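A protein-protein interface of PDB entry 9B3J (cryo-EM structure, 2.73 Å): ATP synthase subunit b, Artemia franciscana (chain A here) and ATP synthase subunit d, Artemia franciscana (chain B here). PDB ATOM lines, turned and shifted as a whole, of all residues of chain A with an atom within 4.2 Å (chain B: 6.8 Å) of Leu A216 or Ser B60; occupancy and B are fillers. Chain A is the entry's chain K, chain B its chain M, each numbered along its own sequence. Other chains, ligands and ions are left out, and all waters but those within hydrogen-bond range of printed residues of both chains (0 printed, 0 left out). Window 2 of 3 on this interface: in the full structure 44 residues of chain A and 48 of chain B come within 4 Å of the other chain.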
ATOM      1  N   LEU A 212       9.929  -4.767   7.562  1.00  0.00           N
ATOM      2  CA  LEU A 212       9.912  -6.105   6.970  1.00  0.00           C
ATOM      3  C   LEU A 212       9.133  -6.127   5.658  1.00  0.00           C
ATOM      4  O   LEU A 212       9.534  -6.803   4.701  1.00  0.00           O
ATOM      5  CB  LEU A 212       9.320  -7.111   7.958  1.00  0.00           C
ATOM      6  CG  LEU A 212      10.292  -7.941   8.801  1.00  0.00           C
ATOM      7  CD1 LEU A 212      11.225  -8.746   7.909  1.00  0.00           C
ATOM      8  CD2 LEU A 212      11.081  -7.070   9.765  1.00  0.00           C
ATOM      9  N   ASP A 213       8.017  -5.394   5.598  1.00  0.00           N
ATOM     10  CA  ASP A 213       7.249  -5.312   4.359  1.00  0.00           C
ATOM     11  C   ASP A 213       8.026  -4.581   3.272  1.00  0.00           C
ATOM     12  O   ASP A 213       7.920  -4.928   2.090  1.00  0.00           O
ATOM     13  CB  ASP A 213       5.909  -4.624   4.614  1.00  0.00           C
ATOM     14  CG  ASP A 213       4.973  -5.466   5.454  1.00  0.00           C
ATOM     15  OD1 ASP A 213       5.356  -6.598   5.821  1.00  0.00           O
ATOM     16  OD2 ASP A 213       3.852  -4.998   5.746  1.00  0.00           O
ATOM     17  N   TYR A 214       8.808  -3.564   3.654  1.00  0.00           N
ATOM     18  CA  TYR A 214       9.649  -2.871   2.681  1.00  0.00           C
ATOM     19  C   TYR A 214      10.722  -3.791   2.113  1.00  0.00           C
ATOM     20  O   TYR A 214      10.995  -3.763   0.905  1.00  0.00           O
ATOM     21  CB  TYR A 214      10.292  -1.643   3.323  1.00  0.00           C
ATOM     22  CG  TYR A 214      11.411  -1.050   2.497  1.00  0.00           C
ATOM     23  CD1 TYR A 214      11.139  -0.298   1.361  1.00  0.00           C
ATOM     24  CD2 TYR A 214      12.743  -1.243   2.852  1.00  0.00           C
ATOM     25  CE1 TYR A 214      12.157   0.246   0.604  1.00  0.00           C
ATOM     26  CE2 TYR A 214      13.766  -0.704   2.101  1.00  0.00           C
ATOM     27  CZ  TYR A 214      13.469   0.039   0.978  1.00  0.00           C
ATOM     28  OH  TYR A 214      14.485   0.579   0.227  1.00  0.00           O
ATOM     29  N   HIS A 215      11.351  -4.599   2.973  1.00  0.00           N
ATOM     30  CA  HIS A 215      12.354  -5.552   2.497  1.00  0.00           C
ATOM     31  C   HIS A 215      11.734  -6.604   1.584  1.00  0.00           C
ATOM     32  O   HIS A 215      12.330  -6.985   0.564  1.00  0.00           O
ATOM     33  CB  HIS A 215      13.051  -6.221   3.680  1.00  0.00           C
ATOM     34  CG  HIS A 215      14.145  -5.397   4.281  1.00  0.00           C
ATOM     35  ND1 HIS A 215      15.403  -5.315   3.726  1.00  0.00           N
ATOM     36  CD2 HIS A 215      14.171  -4.624   5.392  1.00  0.00           C
ATOM     37  CE1 HIS A 215      16.158  -4.525   4.467  1.00  0.00           C
ATOM     38  NE2 HIS A 215      15.435  -4.092   5.484  1.00  0.00           N
ATOM     39  N   LEU A 216      10.535  -7.083   1.934  1.00  0.00           N
ATOM     40  CA  LEU A 216       9.846  -8.062   1.098  1.00  0.00           C
ATOM     41  C   LEU A 216       9.484  -7.480  -0.263  1.00  0.00           C
ATOM     42  O   LEU A 216       9.674  -8.135  -1.295  1.00  0.00           O
ATOM     43  CB  LEU A 216       8.593  -8.567   1.813  1.00  0.00           C
ATOM     44  CG  LEU A 216       7.609  -9.406   0.996  1.00  0.00           C
ATOM     45  CD1 LEU A 216       8.228 -10.732   0.583  1.00  0.00           C
ATOM     46  CD2 LEU A 216       6.321  -9.633   1.774  1.00  0.00           C
ATOM     47  N   GLU A 217       8.972  -6.246  -0.285  1.00  0.00           N
ATOM     48  CA  GLU A 217       8.600  -5.618  -1.548  1.00  0.00           C
ATOM     49  C   GLU A 217       9.822  -5.318  -2.405  1.00  0.00           C
ATOM     50  O   GLU A 217       9.773  -5.470  -3.632  1.00  0.00           O
ATOM     51  CB  GLU A 217       7.801  -4.344  -1.287  1.00  0.00           C
ATOM     52  CG  GLU A 217       6.375  -4.594  -0.832  1.00  0.00           C
ATOM     53  CD  GLU A 217       5.512  -5.196  -1.922  1.00  0.00           C
ATOM     54  OE1 GLU A 217       5.772  -4.919  -3.112  1.00  0.00           O
ATOM     55  OE2 GLU A 217       4.573  -5.948  -1.590  1.00  0.00           O
ATOM     56  N   THR A 218      10.925  -4.892  -1.781  1.00  0.00           N
ATOM     57  CA  THR A 218      12.147  -4.619  -2.531  1.00  0.00           C
ATOM     58  C   THR A 218      12.717  -5.889  -3.150  1.00  0.00           C
ATOM     59  O   THR A 218      13.111  -5.893  -4.327  1.00  0.00           O
ATOM     60  CB  THR A 218      13.181  -3.957  -1.619  1.00  0.00           C
ATOM     61  OG1 THR A 218      12.607  -2.798  -1.003  1.00  0.00           O
ATOM     62  CG2 THR A 218      14.409  -3.543  -2.416  1.00  0.00           C
ATOM     63  N   GLU A 219      12.744  -6.985  -2.383  1.00  0.00           N
ATOM     64  CA  GLU A 219      13.267  -8.241  -2.914  1.00  0.00           C
ATOM     65  C   GLU A 219      12.356  -8.810  -3.995  1.00  0.00           C
ATOM     66  O   GLU A 219      12.839  -9.361  -4.992  1.00  0.00           O
ATOM     67  CB  GLU A 219      13.454  -9.254  -1.786  1.00  0.00           C
ATOM     68  CG  GLU A 219      14.570 -10.256  -2.041  1.00  0.00           C
ATOM     69  CD  GLU A 219      14.392 -11.547  -1.268  1.00  0.00           C
ATOM     70  OE1 GLU A 219      13.359 -12.221  -1.463  1.00  0.00           O
ATOM     71  OE2 GLU A 219      15.284 -11.889  -0.464  1.00  0.00           O
ATOM     72  N   ARG A 220      11.036  -8.677  -3.822  1.00  0.00           N
ATOM     73  CA  ARG A 220      10.102  -9.174  -4.827  1.00  0.00           C
ATOM     74  C   ARG A 220      10.182  -8.361  -6.112  1.00  0.00           C
ATOM     75  O   ARG A 220      10.087  -8.920  -7.211  1.00  0.00           O
ATOM     76  CB  ARG A 220       8.679  -9.157  -4.268  1.00  0.00           C
ATOM     77  CG  ARG A 220       7.659  -9.850  -5.150  1.00  0.00           C
ATOM     78  CD  ARG A 220       6.326  -9.995  -4.438  1.00  0.00           C
ATOM     79  NE  ARG A 220       5.385 -10.804  -5.205  1.00  0.00           N
ATOM     80  CZ  ARG A 220       4.187 -11.170  -4.772  1.00  0.00           C
ATOM     81  NH1 ARG A 220       3.747 -10.819  -3.575  1.00  0.00           N
ATOM     82  NH2 ARG A 220       3.411 -11.909  -5.559  1.00  0.00           N
ATOM     83  N   GLU B  55       8.893 -17.228  10.339  1.00  0.00           N
ATOM     84  CA  GLU B  55       8.958 -18.332   9.387  1.00  0.00           C
ATOM     85  C   GLU B  55       8.337 -17.947   8.050  1.00  0.00           C
ATOM     86  O   GLU B  55       8.824 -18.361   6.990  1.00  0.00           O
ATOM     87  CB  GLU B  55       8.261 -19.564   9.965  1.00  0.00           C
ATOM     88  CG  GLU B  55       8.845 -20.062  11.278  1.00  0.00           C
ATOM     89  CD  GLU B  55      10.173 -20.771  11.103  1.00  0.00           C
ATOM     90  OE1 GLU B  55      10.473 -21.217   9.975  1.00  0.00           O
ATOM     91  OE2 GLU B  55      10.920 -20.885  12.098  1.00  0.00           O
ATOM     92  N   HIS B  56       7.261 -17.157   8.081  1.00  0.00           N
ATOM     93  CA  HIS B  56       6.631 -16.699   6.846  1.00  0.00           C
ATOM     94  C   HIS B  56       7.562 -15.791   6.051  1.00  0.00           C
ATOM     95  O   HIS B  56       7.638 -15.891   4.820  1.00  0.00           O
ATOM     96  CB  HIS B  56       5.322 -15.978   7.161  1.00  0.00           C
ATOM     97  CG  HIS B  56       4.618 -15.452   5.951  1.00  0.00           C
ATOM     98  ND1 HIS B  56       4.168 -16.270   4.938  1.00  0.00           N
ATOM     99  CD2 HIS B  56       4.290 -14.189   5.588  1.00  0.00           C
ATOM    100  CE1 HIS B  56       3.591 -15.535   4.005  1.00  0.00           C
ATOM    101  NE2 HIS B  56       3.652 -14.269   4.375  1.00  0.00           N
ATOM    102  N   TYR B  57       8.284 -14.902   6.738  1.00  0.00           N
ATOM    103  CA  TYR B  57       9.238 -14.040   6.051  1.00  0.00           C
ATOM    104  C   TYR B  57      10.471 -14.810   5.595  1.00  0.00           C
ATOM    105  O   TYR B  57      11.089 -14.440   4.591  1.00  0.00           O
ATOM    106  CB  TYR B  57       9.638 -12.873   6.951  1.00  0.00           C
ATOM    107  CG  TYR B  57       8.561 -11.824   7.077  1.00  0.00           C
ATOM    108  CD1 TYR B  57       8.490 -10.767   6.178  1.00  0.00           C
ATOM    109  CD2 TYR B  57       7.609 -11.893   8.085  1.00  0.00           C
ATOM    110  CE1 TYR B  57       7.505  -9.805   6.285  1.00  0.00           C
ATOM    111  CE2 TYR B  57       6.620 -10.937   8.200  1.00  0.00           C
ATOM    112  CZ  TYR B  57       6.573  -9.894   7.297  1.00  0.00           C
ATOM    113  OH  TYR B  57       5.589  -8.939   7.406  1.00  0.00           O
ATOM    114  N   ARG B  58      10.850 -15.865   6.321  1.00  0.00           N
ATOM    115  CA  ARG B  58      11.930 -16.731   5.857  1.00  0.00           C
ATOM    116  C   ARG B  58      11.540 -17.464   4.580  1.00  0.00           C
ATOM    117  O   ARG B  58      12.363 -17.622   3.671  1.00  0.00           O
ATOM    118  CB  ARG B  58      12.314 -17.731   6.948  1.00  0.00           C
ATOM    119  CG  ARG B  58      13.161 -17.151   8.065  1.00  0.00           C
ATOM    120  CD  ARG B  58      13.452 -18.202   9.122  1.00  0.00           C
ATOM    121  NE  ARG B  58      14.210 -17.663  10.244  1.00  0.00           N
ATOM    122  CZ  ARG B  58      14.615 -18.378  11.285  1.00  0.00           C
ATOM    123  NH1 ARG B  58      14.357 -19.672  11.377  1.00  0.00           N
ATOM    124  NH2 ARG B  58      15.298 -17.779  12.256  1.00  0.00           N
ATOM    125  N   LYS B  59      10.289 -17.923   4.497  1.00  0.00           N
ATOM    126  CA  LYS B  59       9.825 -18.595   3.287  1.00  0.00           C
ATOM    127  C   LYS B  59       9.623 -17.617   2.135  1.00  0.00           C
ATOM    128  O   LYS B  59       9.827 -17.981   0.971  1.00  0.00           O
ATOM    129  CB  LYS B  59       8.529 -19.355   3.566  1.00  0.00           C
ATOM    130  CG  LYS B  59       8.680 -20.516   4.537  1.00  0.00           C
ATOM    131  CD  LYS B  59       7.326 -21.090   4.920  1.00  0.00           C
ATOM    132  CE  LYS B  59       7.466 -22.188   5.959  1.00  0.00           C
ATOM    133  NZ  LYS B  59       6.142 -22.735   6.363  1.00  0.00           N
ATOM    134  N   SER B  60       9.225 -16.382   2.431  1.00  0.00           N
ATOM    135  CA  SER B  60       8.926 -15.398   1.399  1.00  0.00           C
ATOM    136  C   SER B  60      10.151 -14.622   0.931  1.00  0.00           C
ATOM    137  O   SER B  60      10.037 -13.825  -0.006  1.00  0.00           O
ATOM    138  CB  SER B  60       7.860 -14.418   1.898  1.00  0.00           C
ATOM    139  OG  SER B  60       6.659 -15.094   2.224  1.00  0.00           O
ATOM    140  N   LEU B  61      11.311 -14.825   1.550  1.00  0.00           N
ATOM    141  CA  LEU B  61      12.540 -14.153   1.152  1.00  0.00           C
ATOM    142  C   LEU B  61      13.606 -15.182   0.809  1.00  0.00           C
ATOM    143  O   LEU B  61      13.747 -16.198   1.499  1.00  0.00           O
ATOM    144  CB  LEU B  61      13.053 -13.219   2.254  1.00  0.00           C
ATOM    145  CG  LEU B  61      12.191 -11.997   2.575  1.00  0.00           C
ATOM    146  CD1 LEU B  61      12.886 -11.098   3.582  1.00  0.00           C
ATOM    147  CD2 LEU B  61      11.865 -11.228   1.310  1.00  0.00           C
ATOM    148  N   THR B  62      14.345 -14.914  -0.271  1.00  0.00           N
ATOM    149  CA  THR B  62      15.435 -15.799  -0.672  1.00  0.00           C
ATOM    150  C   THR B  62      16.550 -15.809   0.367  1.00  0.00           C
ATOM    151  O   THR B  62      17.090 -16.870   0.697  1.00  0.00           O
ATOM    152  CB  THR B  62      15.975 -15.374  -2.040  1.00  0.00           C
ATOM    153  OG1 THR B  62      14.900 -15.334  -2.987  1.00  0.00           O
ATOM    154  CG2 THR B  62      17.035 -16.350  -2.530  1.00  0.00           C
ATOM    155  N   ASN B  63      16.893 -14.641   0.908  1.00  0.00           N
ATOM    156  CA  ASN B  63      17.918 -14.549   1.934  1.00  0.00           C
ATOM    157  C   ASN B  63      17.245 -14.329   3.278  1.00  0.00           C
ATOM    158  O   ASN B  63      16.729 -13.227   3.527  1.00  0.00           O
ATOM    159  CB  ASN B  63      18.889 -13.410   1.628  1.00  0.00           C
ATOM    160  CG  ASN B  63      20.228 -13.572   2.334  1.00  0.00           C
ATOM    161  OD1 ASN B  63      20.315 -14.182   3.399  1.00  0.00           O
ATOM    162  ND2 ASN B  63      21.278 -13.023   1.737  1.00  0.00           N
ATOM    163  N   MET B  66      18.254 -11.347   6.812  1.00  0.00           N
ATOM    164  CA  MET B  66      17.604 -10.111   7.235  1.00  0.00           C
ATOM    165  C   MET B  66      16.483 -10.389   8.229  1.00  0.00           C
ATOM    166  O   MET B  66      16.289  -9.627   9.182  1.00  0.00           O
ATOM    167  CB  MET B  66      17.068  -9.358   6.018  1.00  0.00           C
ATOM    168  CG  MET B  66      18.130  -8.998   4.993  1.00  0.00           C
ATOM    169  SD  MET B  66      17.432  -8.191   3.541  1.00  0.00           S
ATOM    170  CE  MET B  66      16.310  -9.461   2.958  1.00  0.00           C
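The side-chain hydroxyl (OH) of Tyr B57 sits at hydrogen-bond distance from the side-chain carboxylate (OD1) of Asp A213, at 2.8 Å. The side-chain sulfur of Met B66 sits at hydrogen-bond distance from a ring nitrogen (ND1) of His A215 (3.5 Å). OE1 of Glu A219 lies within hydrogen-bond range of N of Thr B62, at 3.1 Å. The side-chain carboxylate (OE2) of Glu A219 sits at hydrogen-bond distance from the backbone NH (N) of Asn B63.
OG of Ser B60 is in hydrogen-bond range of O of His B56 (2.9 Å).
Tyr B57 touches Leu A212 (CE1 to CB, 3.7 Å). CD1 of Leu A216 touches O of Ser B60 (3.6 Å). Leu A216 touches Leu B61. O of Ser B60 touches OE1 of Glu A219, 3.97 Å away. CD2 of Leu B61 touches OE1 of Glu A219, at 3.3 Å.
Printed residues of chain B within 4 Å of Leu A212: Tyr B57 (3.7 Å). Of the printed residues of chain B, Asp A213 touches Tyr B57 (2.8 Å). Of the printed residues of chain B, His A215 touches Met B66 (3.5 Å). Leu A216 touches two residues of chain B. Glu A217 touches none of the printed residues of chain B. Of the printed residues of chain A, Ser B60 touches Leu A216 (3.6 Å) and Glu A219 (3.97 Å). Of the printed residues of chain A, Asn B63 touches Glu A219 (3.5 Å). Printed residues of chain A within 4 Å of Met B66: His A215. The nearest printed residue of chain A that does not touch Ser B60 is Arg A220 (6.5 Å).
Of the 9 printed residues of chain A, 5 touch a printed residue of chain B. Printed residues of chain A that touch a printed residue of chain B: Leu A212, Asp A213, His A215, Leu A216 and Glu A219. Hydrophobic or aromatic side chains of chain A that line the printed part of chain B: Leu A212, His A215 and Leu A216. Printed residues of chain B that touch a printed residue of chain A: Tyr B57, Ser B60, Leu B61, Thr B62, Asn B63 and Met B66. Hydrophobic or aromatic side chains of chain B within 4 Å of the printed part of chain A: Tyr B57, Leu B61 and Met B66. Among the printed residues, no Asp or Glu carboxylate lies within 4 Å of a Lys or Arg side-chain nitrogen of the other chain.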
